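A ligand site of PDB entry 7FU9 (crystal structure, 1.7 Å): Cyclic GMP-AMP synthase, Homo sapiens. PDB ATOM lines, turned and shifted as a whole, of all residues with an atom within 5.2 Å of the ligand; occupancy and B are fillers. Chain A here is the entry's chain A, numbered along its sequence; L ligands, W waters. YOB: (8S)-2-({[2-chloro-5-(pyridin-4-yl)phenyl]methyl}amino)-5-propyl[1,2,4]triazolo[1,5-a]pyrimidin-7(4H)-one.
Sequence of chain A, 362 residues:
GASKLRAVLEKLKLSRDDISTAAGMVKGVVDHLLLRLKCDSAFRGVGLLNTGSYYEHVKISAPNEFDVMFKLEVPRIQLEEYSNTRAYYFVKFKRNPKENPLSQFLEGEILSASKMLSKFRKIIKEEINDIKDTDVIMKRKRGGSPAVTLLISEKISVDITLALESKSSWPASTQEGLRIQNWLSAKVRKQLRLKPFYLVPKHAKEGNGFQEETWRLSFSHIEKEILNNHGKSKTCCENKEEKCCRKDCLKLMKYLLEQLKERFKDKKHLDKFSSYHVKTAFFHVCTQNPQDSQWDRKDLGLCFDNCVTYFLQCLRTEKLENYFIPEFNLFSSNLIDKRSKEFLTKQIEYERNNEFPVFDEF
OH of Tyr 276 sits at hydrogen-bond distance from ND2 of Asn 322, 2.7 Å away. The backbone NH (N) of Asn 322 is in hydrogen-bond range of the backbone carbonyl oxygen (O) of Phe 328. N of Ile 325 is in hydrogen-bond range of OD1 of Asn 322. N of Phe 324 sits at hydrogen-bond distance from OD1 of Asn 322. O of Tyr 276 sits at hydrogen-bond distance from OG1 of Thr 280 (2.9 Å). NH2 of Arg 216 is in hydrogen-bond range of OG of Ser 145 (3.3 Å). NZ of Lys 279 is in salt-bridge range of OE2 of Glu 223 (2.9 Å). OH of Tyr 323 lies within hydrogen-bond range of O of Phe 283 (3.2 Å).
O20 of the ligand lies within hydrogen-bond range of N of Ser 220 (2.9 Å). The backbone carbonyl oxygen of Leu 217 lies within hydrogen-bond range of a nitrogen (N15) of the ligand (3.0 Å). A nitrogen (N25) of the ligand sits at hydrogen-bond distance from the side-chain amide nitrogen (ND2) of Asn 322, 3.0 Å away. N17 of the ligand lies within hydrogen-bond range of N of Phe 219, 3.1 Å away.
Water W3 lies within hydrogen-bond range of an oxygen (O20) of the ligand, the side-chain hydroxyl (OG) of Ser 220 and the side-chain carboxylate (OE1) of Glu 223. Water W2 lies within hydrogen-bond range of the side-chain hydroxyl of Ser 218 (2.7 Å), an oxygen (O20) of the ligand (2.8 Å) and the guanidinium group of Arg 216 (3.3 Å).
Ala 87 touches the ligand. Arg 216 touches the ligand (NH1 to C10, 3.3 Å). Ser 218 touches the ligand (CA to N17, 3.6 Å). OE1 of Glu 223 touches C21 of the ligand, at 3.5 Å. OH of Tyr 276 touches C4 of the ligand, at 3.2 Å. OG1 of Thr 280 touches C26 of the ligand (3.99 Å). Phe 283 touches the ligand (CD2 to C28, 3.7 Å). CB of Tyr 323 touches C27 of the ligand, at 3.8 Å. CE1 of Phe 324 touches C28 of the ligand (3.6 Å). CD1 of Ile 325 touches CL8 of the ligand (3.6 Å). Phe 328 touches the ligand (CE1 to C6, 3.6 Å). Hydrophobic or aromatic side chains that line the ligand: Ala 87, Phe 219, Tyr 276, Phe 283, Tyr 323, Phe 324, Ile 325 and Phe 328. Of the 21 residues printed, 15 come within 4 Å of the ligand. The nearest printed residue that does not touch the ligand is Ile 226 (4.4 Å).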
ATOM      1  N   ALA A  87     -21.877  12.446  -8.206  1.00  0.00           N
ATOM      2  CA  ALA A  87     -21.737  11.124  -8.794  1.00  0.00           C
ATOM      3  C   ALA A  87     -21.030  10.107  -7.905  1.00  0.00           C
ATOM      4  O   ALA A  87     -21.307   8.905  -8.023  1.00  0.00           O
ATOM      5  CB  ALA A  87     -20.979  11.232 -10.121  1.00  0.00           C
ATOM      6  N   TYR A  88     -20.115  10.534  -7.032  1.00  0.00           N
ATOM      7  CA  TYR A  88     -19.233   9.633  -6.313  1.00  0.00           C
ATOM      8  C   TYR A  88     -19.522   9.672  -4.811  1.00  0.00           C
ATOM      9  O   TYR A  88     -19.826  10.721  -4.248  1.00  0.00           O
ATOM     10  CB  TYR A  88     -17.767   9.971  -6.592  1.00  0.00           C
ATOM     11  CG  TYR A  88     -17.407   9.885  -8.069  1.00  0.00           C
ATOM     12  CD1 TYR A  88     -17.520  10.995  -8.894  1.00  0.00           C
ATOM     13  CD2 TYR A  88     -16.954   8.685  -8.624  1.00  0.00           C
ATOM     14  CE1 TYR A  88     -17.211  10.918 -10.250  1.00  0.00           C
ATOM     15  CE2 TYR A  88     -16.635   8.598  -9.978  1.00  0.00           C
ATOM     16  CZ  TYR A  88     -16.760   9.718 -10.791  1.00  0.00           C
ATOM     17  OH  TYR A  88     -16.450   9.624 -12.132  1.00  0.00           O
ATOM     18  N   SER A 145     -13.298   1.531 -13.669  1.00  0.00           N
ATOM     19  CA  SER A 145     -14.734   1.295 -13.781  1.00  0.00           C
ATOM     20  C   SER A 145     -15.045   0.005 -14.530  1.00  0.00           C
ATOM     21  O   SER A 145     -15.896  -0.764 -14.041  1.00  0.00           O
ATOM     22  CB  SER A 145     -15.415   2.512 -14.427  1.00  0.00           C
ATOM     23  OG  SER A 145     -16.825   2.358 -14.486  1.00  0.00           O
ATOM     24  N   LYS A 202     -15.457   3.310  -9.215  1.00  0.00           N
ATOM     25  CA  LYS A 202     -14.668   4.160 -10.099  1.00  0.00           C
ATOM     26  C   LYS A 202     -13.998   5.253  -9.284  1.00  0.00           C
ATOM     27  O   LYS A 202     -14.522   5.715  -8.270  1.00  0.00           O
ATOM     28  CB  LYS A 202     -15.526   4.799 -11.203  1.00  0.00           C
ATOM     29  CG  LYS A 202     -14.680   5.498 -12.263  1.00  0.00           C
ATOM     30  CD  LYS A 202     -15.489   6.392 -13.178  1.00  0.00           C
ATOM     31  CE  LYS A 202     -14.546   7.124 -14.126  1.00  0.00           C
ATOM     32  NZ  LYS A 202     -15.270   7.867 -15.206  1.00  0.00           N
ATOM     33  N   ARG A 216     -19.210   4.992  -7.800  1.00  0.00           N
ATOM     34  CA  ARG A 216     -20.104   5.739  -8.674  1.00  0.00           C
ATOM     35  C   ARG A 216     -21.425   4.993  -8.819  1.00  0.00           C
ATOM     36  O   ARG A 216     -21.469   3.752  -8.784  1.00  0.00           O
ATOM     37  CB  ARG A 216     -19.438   5.988 -10.044  1.00  0.00           C
ATOM     38  CG  ARG A 216     -20.390   6.159 -11.203  1.00  0.00           C
ATOM     39  CD  ARG A 216     -19.719   6.163 -12.589  1.00  0.00           C
ATOM     40  NE  ARG A 216     -19.496   4.842 -13.181  1.00  0.00           N
ATOM     41  CZ  ARG A 216     -20.449   4.004 -13.624  1.00  0.00           C
ATOM     42  NH1 ARG A 216     -21.739   4.279 -13.524  1.00  0.00           N
ATOM     43  NH2 ARG A 216     -20.090   2.854 -14.164  1.00  0.00           N
ATOM     44  N   LEU A 217     -22.522   5.729  -8.965  1.00  0.00           N
ATOM     45  CA  LEU A 217     -23.816   5.107  -9.187  1.00  0.00           C
ATOM     46  C   LEU A 217     -23.902   4.508 -10.594  1.00  0.00           C
ATOM     47  O   LEU A 217     -23.243   4.983 -11.533  1.00  0.00           O
ATOM     48  CB  LEU A 217     -24.954   6.113  -8.985  1.00  0.00           C
ATOM     49  CG  LEU A 217     -25.018   6.826  -7.635  1.00  0.00           C
ATOM     50  CD1 LEU A 217     -26.245   7.729  -7.608  1.00  0.00           C
ATOM     51  CD2 LEU A 217     -25.059   5.821  -6.497  1.00  0.00           C
ATOM     52  N   SER A 218     -24.720   3.469 -10.731  1.00  0.00           N
ATOM     53  CA  SER A 218     -24.912   2.804 -12.010  1.00  0.00           C
ATOM     54  C   SER A 218     -26.380   2.437 -12.188  1.00  0.00           C
ATOM     55  O   SER A 218     -27.027   1.952 -11.261  1.00  0.00           O
ATOM     56  CB  SER A 218     -24.040   1.542 -12.122  1.00  0.00           C
ATOM     57  OG  SER A 218     -24.322   0.831 -13.319  1.00  0.00           O
ATOM     58  N   PHE A 219     -26.909   2.657 -13.390  1.00  0.00           N
ATOM     59  CA  PHE A 219     -28.316   2.413 -13.676  1.00  0.00           C
ATOM     60  C   PHE A 219     -28.477   1.590 -14.955  1.00  0.00           C
ATOM     61  O   PHE A 219     -29.453   1.749 -15.696  1.00  0.00           O
ATOM     62  CB  PHE A 219     -29.081   3.732 -13.750  1.00  0.00           C
ATOM     63  CG  PHE A 219     -29.138   4.457 -12.435  1.00  0.00           C
ATOM     64  CD1 PHE A 219     -30.148   4.152 -11.517  1.00  0.00           C
ATOM     65  CD2 PHE A 219     -28.195   5.418 -12.102  1.00  0.00           C
ATOM     66  CE1 PHE A 219     -30.196   4.806 -10.278  1.00  0.00           C
ATOM     67  CE2 PHE A 219     -28.238   6.083 -10.883  1.00  0.00           C
ATOM     68  CZ  PHE A 219     -29.238   5.769  -9.964  1.00  0.00           C
ATOM     69  N   SER A 220     -27.533   0.668 -15.184  1.00  0.00           N
ATOM     70  CA  SER A 220     -27.549  -0.169 -16.379  1.00  0.00           C
ATOM     71  C   SER A 220     -28.868  -0.915 -16.538  1.00  0.00           C
ATOM     72  O   SER A 220     -29.369  -1.074 -17.659  1.00  0.00           O
ATOM     73  CB  SER A 220     -26.379  -1.154 -16.312  1.00  0.00           C
ATOM     74  OG  SER A 220     -25.995  -1.556 -17.603  1.00  0.00           O
ATOM     75  N   GLU A 223     -31.506   1.463 -18.052  1.00  0.00           N
ATOM     76  CA  GLU A 223     -31.307   1.675 -19.477  1.00  0.00           C
ATOM     77  C   GLU A 223     -31.961   0.567 -20.297  1.00  0.00           C
ATOM     78  O   GLU A 223     -32.720   0.830 -21.238  1.00  0.00           O
ATOM     79  CB  GLU A 223     -29.807   1.754 -19.782  1.00  0.00           C
ATOM     80  CG  GLU A 223     -29.487   1.797 -21.274  1.00  0.00           C
ATOM     81  CD  GLU A 223     -28.022   1.526 -21.565  1.00  0.00           C
ATOM     82  OE1 GLU A 223     -27.152   2.045 -20.842  1.00  0.00           O
ATOM     83  OE2 GLU A 223     -27.741   0.774 -22.521  1.00  0.00           O
ATOM     84  N   ILE A 226     -35.887   0.876 -20.232  1.00  0.00           N
ATOM     85  CA  ILE A 226     -36.497   1.954 -21.017  1.00  0.00           C
ATOM     86  C   ILE A 226     -36.165   1.869 -22.505  1.00  0.00           C
ATOM     87  O   ILE A 226     -36.759   2.604 -23.296  1.00  0.00           O
ATOM     88  CB  ILE A 226     -36.126   3.389 -20.554  1.00  0.00           C
ATOM     89  CG1 ILE A 226     -34.638   3.710 -20.751  1.00  0.00           C
ATOM     90  CG2 ILE A 226     -36.558   3.644 -19.061  1.00  0.00           C
ATOM     91  CD1 ILE A 226     -34.264   5.124 -20.252  1.00  0.00           C
ATOM     92  N   TYR A 276     -21.664   5.525 -24.438  1.00  0.00           N
ATOM     93  CA  TYR A 276     -22.342   6.080 -23.261  1.00  0.00           C
ATOM     94  C   TYR A 276     -22.783   7.533 -23.493  1.00  0.00           C
ATOM     95  O   TYR A 276     -23.875   7.940 -23.076  1.00  0.00           O
ATOM     96  CB  TYR A 276     -21.425   5.964 -22.036  1.00  0.00           C
ATOM     97  CG  TYR A 276     -21.840   6.825 -20.864  1.00  0.00           C
ATOM     98  CD1 TYR A 276     -23.069   6.632 -20.228  1.00  0.00           C
ATOM     99  CD2 TYR A 276     -21.002   7.833 -20.396  1.00  0.00           C
ATOM    100  CE1 TYR A 276     -23.463   7.440 -19.152  1.00  0.00           C
ATOM    101  CE2 TYR A 276     -21.383   8.642 -19.325  1.00  0.00           C
ATOM    102  CZ  TYR A 276     -22.611   8.438 -18.710  1.00  0.00           C
ATOM    103  OH  TYR A 276     -22.989   9.230 -17.639  1.00  0.00           O
ATOM    104  N   LYS A 279     -25.720   7.365 -26.070  1.00  0.00           N
ATOM    105  CA  LYS A 279     -26.942   6.893 -25.421  1.00  0.00           C
ATOM    106  C   LYS A 279     -27.576   7.998 -24.575  1.00  0.00           C
ATOM    107  O   LYS A 279     -28.792   8.136 -24.549  1.00  0.00           O
ATOM    108  CB  LYS A 279     -26.648   5.705 -24.507  1.00  0.00           C
ATOM    109  CG  LYS A 279     -26.459   4.370 -25.166  1.00  0.00           C
ATOM    110  CD  LYS A 279     -25.848   3.419 -24.134  1.00  0.00           C
ATOM    111  CE  LYS A 279     -25.750   2.000 -24.634  1.00  0.00           C
ATOM    112  NZ  LYS A 279     -25.103   1.167 -23.584  1.00  0.00           N
ATOM    113  N   THR A 280     -26.755   8.733 -23.820  1.00  0.00           N
ATOM    114  CA  THR A 280     -27.277   9.781 -22.965  1.00  0.00           C
ATOM    115  C   THR A 280     -28.019  10.824 -23.781  1.00  0.00           C
ATOM    116  O   THR A 280     -29.149  11.210 -23.461  1.00  0.00           O
ATOM    117  CB  THR A 280     -26.128  10.420 -22.142  1.00  0.00           C
ATOM    118  OG1 THR A 280     -25.565   9.437 -21.273  1.00  0.00           O
ATOM    119  CG2 THR A 280     -26.633  11.581 -21.301  1.00  0.00           C
ATOM    120  N   PHE A 283     -31.433   9.454 -25.147  1.00  0.00           N
ATOM    121  CA  PHE A 283     -32.533   9.447 -24.175  1.00  0.00           C
ATOM    122  C   PHE A 283     -33.023  10.850 -23.821  1.00  0.00           C
ATOM    123  O   PHE A 283     -34.210  11.026 -23.528  1.00  0.00           O
ATOM    124  CB  PHE A 283     -32.146   8.679 -22.912  1.00  0.00           C
ATOM    125  CG  PHE A 283     -32.116   7.207 -23.113  1.00  0.00           C
ATOM    126  CD1 PHE A 283     -33.290   6.515 -23.403  1.00  0.00           C
ATOM    127  CD2 PHE A 283     -30.928   6.506 -23.070  1.00  0.00           C
ATOM    128  CE1 PHE A 283     -33.256   5.155 -23.613  1.00  0.00           C
ATOM    129  CE2 PHE A 283     -30.911   5.132 -23.267  1.00  0.00           C
ATOM    130  CZ  PHE A 283     -32.070   4.478 -23.528  1.00  0.00           C
ATOM    131  N   ASN A 322     -25.792  14.140 -17.410  1.00  0.00           N
ATOM    132  CA  ASN A 322     -26.129  12.771 -17.048  1.00  0.00           C
ATOM    133  C   ASN A 322     -27.644  12.613 -16.915  1.00  0.00           C
ATOM    134  O   ASN A 322     -28.319  13.462 -16.327  1.00  0.00           O
ATOM    135  CB  ASN A 322     -25.419  12.385 -15.748  1.00  0.00           C
ATOM    136  CG  ASN A 322     -25.676  10.947 -15.367  1.00  0.00           C
ATOM    137  OD1 ASN A 322     -26.626  10.650 -14.656  1.00  0.00           O
ATOM    138  ND2 ASN A 322     -24.848  10.049 -15.883  1.00  0.00           N
ATOM    139  N   TYR A 323     -28.172  11.500 -17.454  1.00  0.00           N
ATOM    140  CA  TYR A 323     -29.615  11.264 -17.509  1.00  0.00           C
ATOM    141  C   TYR A 323     -30.244  11.133 -16.122  1.00  0.00           C
ATOM    142  O   TYR A 323     -31.431  11.451 -15.945  1.00  0.00           O
ATOM    143  CB  TYR A 323     -29.906  10.004 -18.328  1.00  0.00           C
ATOM    144  CG  TYR A 323     -31.307  10.031 -18.910  1.00  0.00           C
ATOM    145  CD1 TYR A 323     -31.662  11.022 -19.815  1.00  0.00           C
ATOM    146  CD2 TYR A 323     -32.272   9.105 -18.526  1.00  0.00           C
ATOM    147  CE1 TYR A 323     -32.935  11.071 -20.345  1.00  0.00           C
ATOM    148  CE2 TYR A 323     -33.559   9.127 -19.078  1.00  0.00           C
ATOM    149  CZ  TYR A 323     -33.883  10.130 -19.980  1.00  0.00           C
ATOM    150  OH  TYR A 323     -35.139  10.209 -20.550  1.00  0.00           O
ATOM    151  N   PHE A 324     -29.467  10.675 -15.146  1.00  0.00           N
ATOM    152  CA  PHE A 324     -29.962  10.441 -13.790  1.00  0.00           C
ATOM    153  C   PHE A 324     -29.553  11.505 -12.795  1.00  0.00           C
ATOM    154  O   PHE A 324     -30.285  11.756 -11.834  1.00  0.00           O
ATOM    155  CB  PHE A 324     -29.484   9.062 -13.296  1.00  0.00           C
ATOM    156  CG  PHE A 324     -30.014   7.928 -14.106  1.00  0.00           C
ATOM    157  CD1 PHE A 324     -29.379   7.530 -15.278  1.00  0.00           C
ATOM    158  CD2 PHE A 324     -31.170   7.281 -13.731  1.00  0.00           C
ATOM    159  CE1 PHE A 324     -29.874   6.496 -16.042  1.00  0.00           C
ATOM    160  CE2 PHE A 324     -31.684   6.250 -14.484  1.00  0.00           C
ATOM    161  CZ  PHE A 324     -31.048   5.865 -15.648  1.00  0.00           C
ATOM    162  N   ILE A 325     -28.388  12.120 -12.976  1.00  0.00           N
ATOM    163  CA  ILE A 325     -27.890  13.164 -12.090  1.00  0.00           C
ATOM    164  C   ILE A 325     -27.630  14.386 -12.945  1.00  0.00           C
ATOM    165  O   ILE A 325     -26.533  14.506 -13.534  1.00  0.00           O
ATOM    166  CB  ILE A 325     -26.630  12.705 -11.349  1.00  0.00           C
ATOM    167  CG1 ILE A 325     -26.928  11.392 -10.598  1.00  0.00           C
ATOM    168  CG2 ILE A 325     -26.108  13.836 -10.447  1.00  0.00           C
ATOM    169  CD1 ILE A 325     -25.800  10.893  -9.724  1.00  0.00           C
ATOM    170  N   PHE A 328     -24.408  16.603 -13.123  1.00  0.00           N
ATOM    171  CA  PHE A 328     -23.164  16.025 -13.624  1.00  0.00           C
ATOM    172  C   PHE A 328     -23.074  16.229 -15.128  1.00  0.00           C
ATOM    173  O   PHE A 328     -23.857  15.641 -15.888  1.00  0.00           O
ATOM    174  CB  PHE A 328     -23.056  14.539 -13.293  1.00  0.00           C
ATOM    175  CG  PHE A 328     -21.666  14.003 -13.469  1.00  0.00           C
ATOM    176  CD1 PHE A 328     -21.222  13.577 -14.715  1.00  0.00           C
ATOM    177  CD2 PHE A 328     -20.788  13.974 -12.401  1.00  0.00           C
ATOM    178  CE1 PHE A 328     -19.931  13.124 -14.876  1.00  0.00           C
ATOM    179  CE2 PHE A 328     -19.501  13.510 -12.555  1.00  0.00           C
ATOM    180  CZ  PHE A 328     -19.071  13.082 -13.782  1.00  0.00           C
ATOM    181  N   LEU A 330     -21.306  15.522 -18.482  1.00  0.00           N
ATOM    182  CA  LEU A 330     -20.392  14.598 -19.150  1.00  0.00           C
ATOM    183  C   LEU A 330     -19.387  15.318 -20.047  1.00  0.00           C
ATOM    184  O   LEU A 330     -18.287  14.808 -20.275  1.00  0.00           O
ATOM    185  CB  LEU A 330     -21.175  13.579 -19.989  1.00  0.00           C
ATOM    186  CG  LEU A 330     -22.328  12.784 -19.362  1.00  0.00           C
ATOM    187  CD1 LEU A 330     -22.846  11.711 -20.306  1.00  0.00           C
ATOM    188  CD2 LEU A 330     -21.859  12.159 -18.075  1.00  0.00           C
HETATM  189  C10 YOB L   1     -21.293   5.758 -16.428  1.00  0.00           C
HETATM  190  C11 YOB L   1     -20.637   4.918 -17.296  1.00  0.00           C
HETATM  191  C13 YOB L   1     -18.906   6.366 -17.535  1.00  0.00           C
HETATM  192  C16 YOB L   1     -25.320   6.253 -14.567  1.00  0.00           C
HETATM  193  C19 YOB L   1     -26.322   3.988 -16.950  1.00  0.00           C
HETATM  194  C21 YOB L   1     -26.838   4.389 -18.225  1.00  0.00           C
HETATM  195  C22 YOB L   1     -26.936   5.699 -18.594  1.00  0.00           C
HETATM  196  C24 YOB L   1     -26.088   6.372 -16.485  1.00  0.00           C
HETATM  197  C26 YOB L   1     -27.452   6.204 -19.906  1.00  0.00           C
HETATM  198  C27 YOB L   1     -28.884   6.729 -19.872  1.00  0.00           C
HETATM  199  C28 YOB L   1     -29.942   5.667 -19.591  1.00  0.00           C
HETATM  200  C1  YOB L   1     -23.265   8.467 -13.711  1.00  0.00           C
HETATM  201  C14 YOB L   1     -19.494   7.280 -16.680  1.00  0.00           C
HETATM  202  C2  YOB L   1     -24.607   8.092 -13.094  1.00  0.00           C
HETATM  203  C3  YOB L   1     -22.597   7.601 -14.578  1.00  0.00           C
HETATM  204  C4  YOB L   1     -21.380   7.928 -15.161  1.00  0.00           C
HETATM  205  C5  YOB L   1     -20.808   9.150 -14.846  1.00  0.00           C
HETATM  206  C6  YOB L   1     -21.433  10.017 -13.988  1.00  0.00           C
HETATM  207  C7  YOB L   1     -22.645   9.673 -13.418  1.00  0.00           C
HETATM  208  C9  YOB L   1     -20.715   6.987 -16.098  1.00  0.00           C
HETATM  209  N12 YOB L   1     -19.457   5.193 -17.855  1.00  0.00           N
HETATM  210  N15 YOB L   1     -24.833   6.687 -13.366  1.00  0.00           N
HETATM  211  N17 YOB L   1     -25.467   4.971 -14.866  1.00  0.00           N
HETATM  212  N18 YOB L   1     -25.971   5.076 -16.142  1.00  0.00           N
HETATM  213  N23 YOB L   1     -26.561   6.695 -17.703  1.00  0.00           N
HETATM  214  N25 YOB L   1     -25.676   7.166 -15.521  1.00  0.00           N
HETATM  215  O20 YOB L   1     -26.172   2.834 -16.533  1.00  0.00           O
HETATM  216 CL8  YOB L   1     -23.408  10.812 -12.369  1.00  0.00          CL
HETATM  217  O   HOH W   1     -26.509   9.356 -18.609  1.00  0.00           O
HETATM  218  O   HOH W   2     -23.655   2.381 -15.451  1.00  0.00           O
HETATM  219  O   HOH W   3     -25.438   1.251 -18.507  1.00  0.00           O
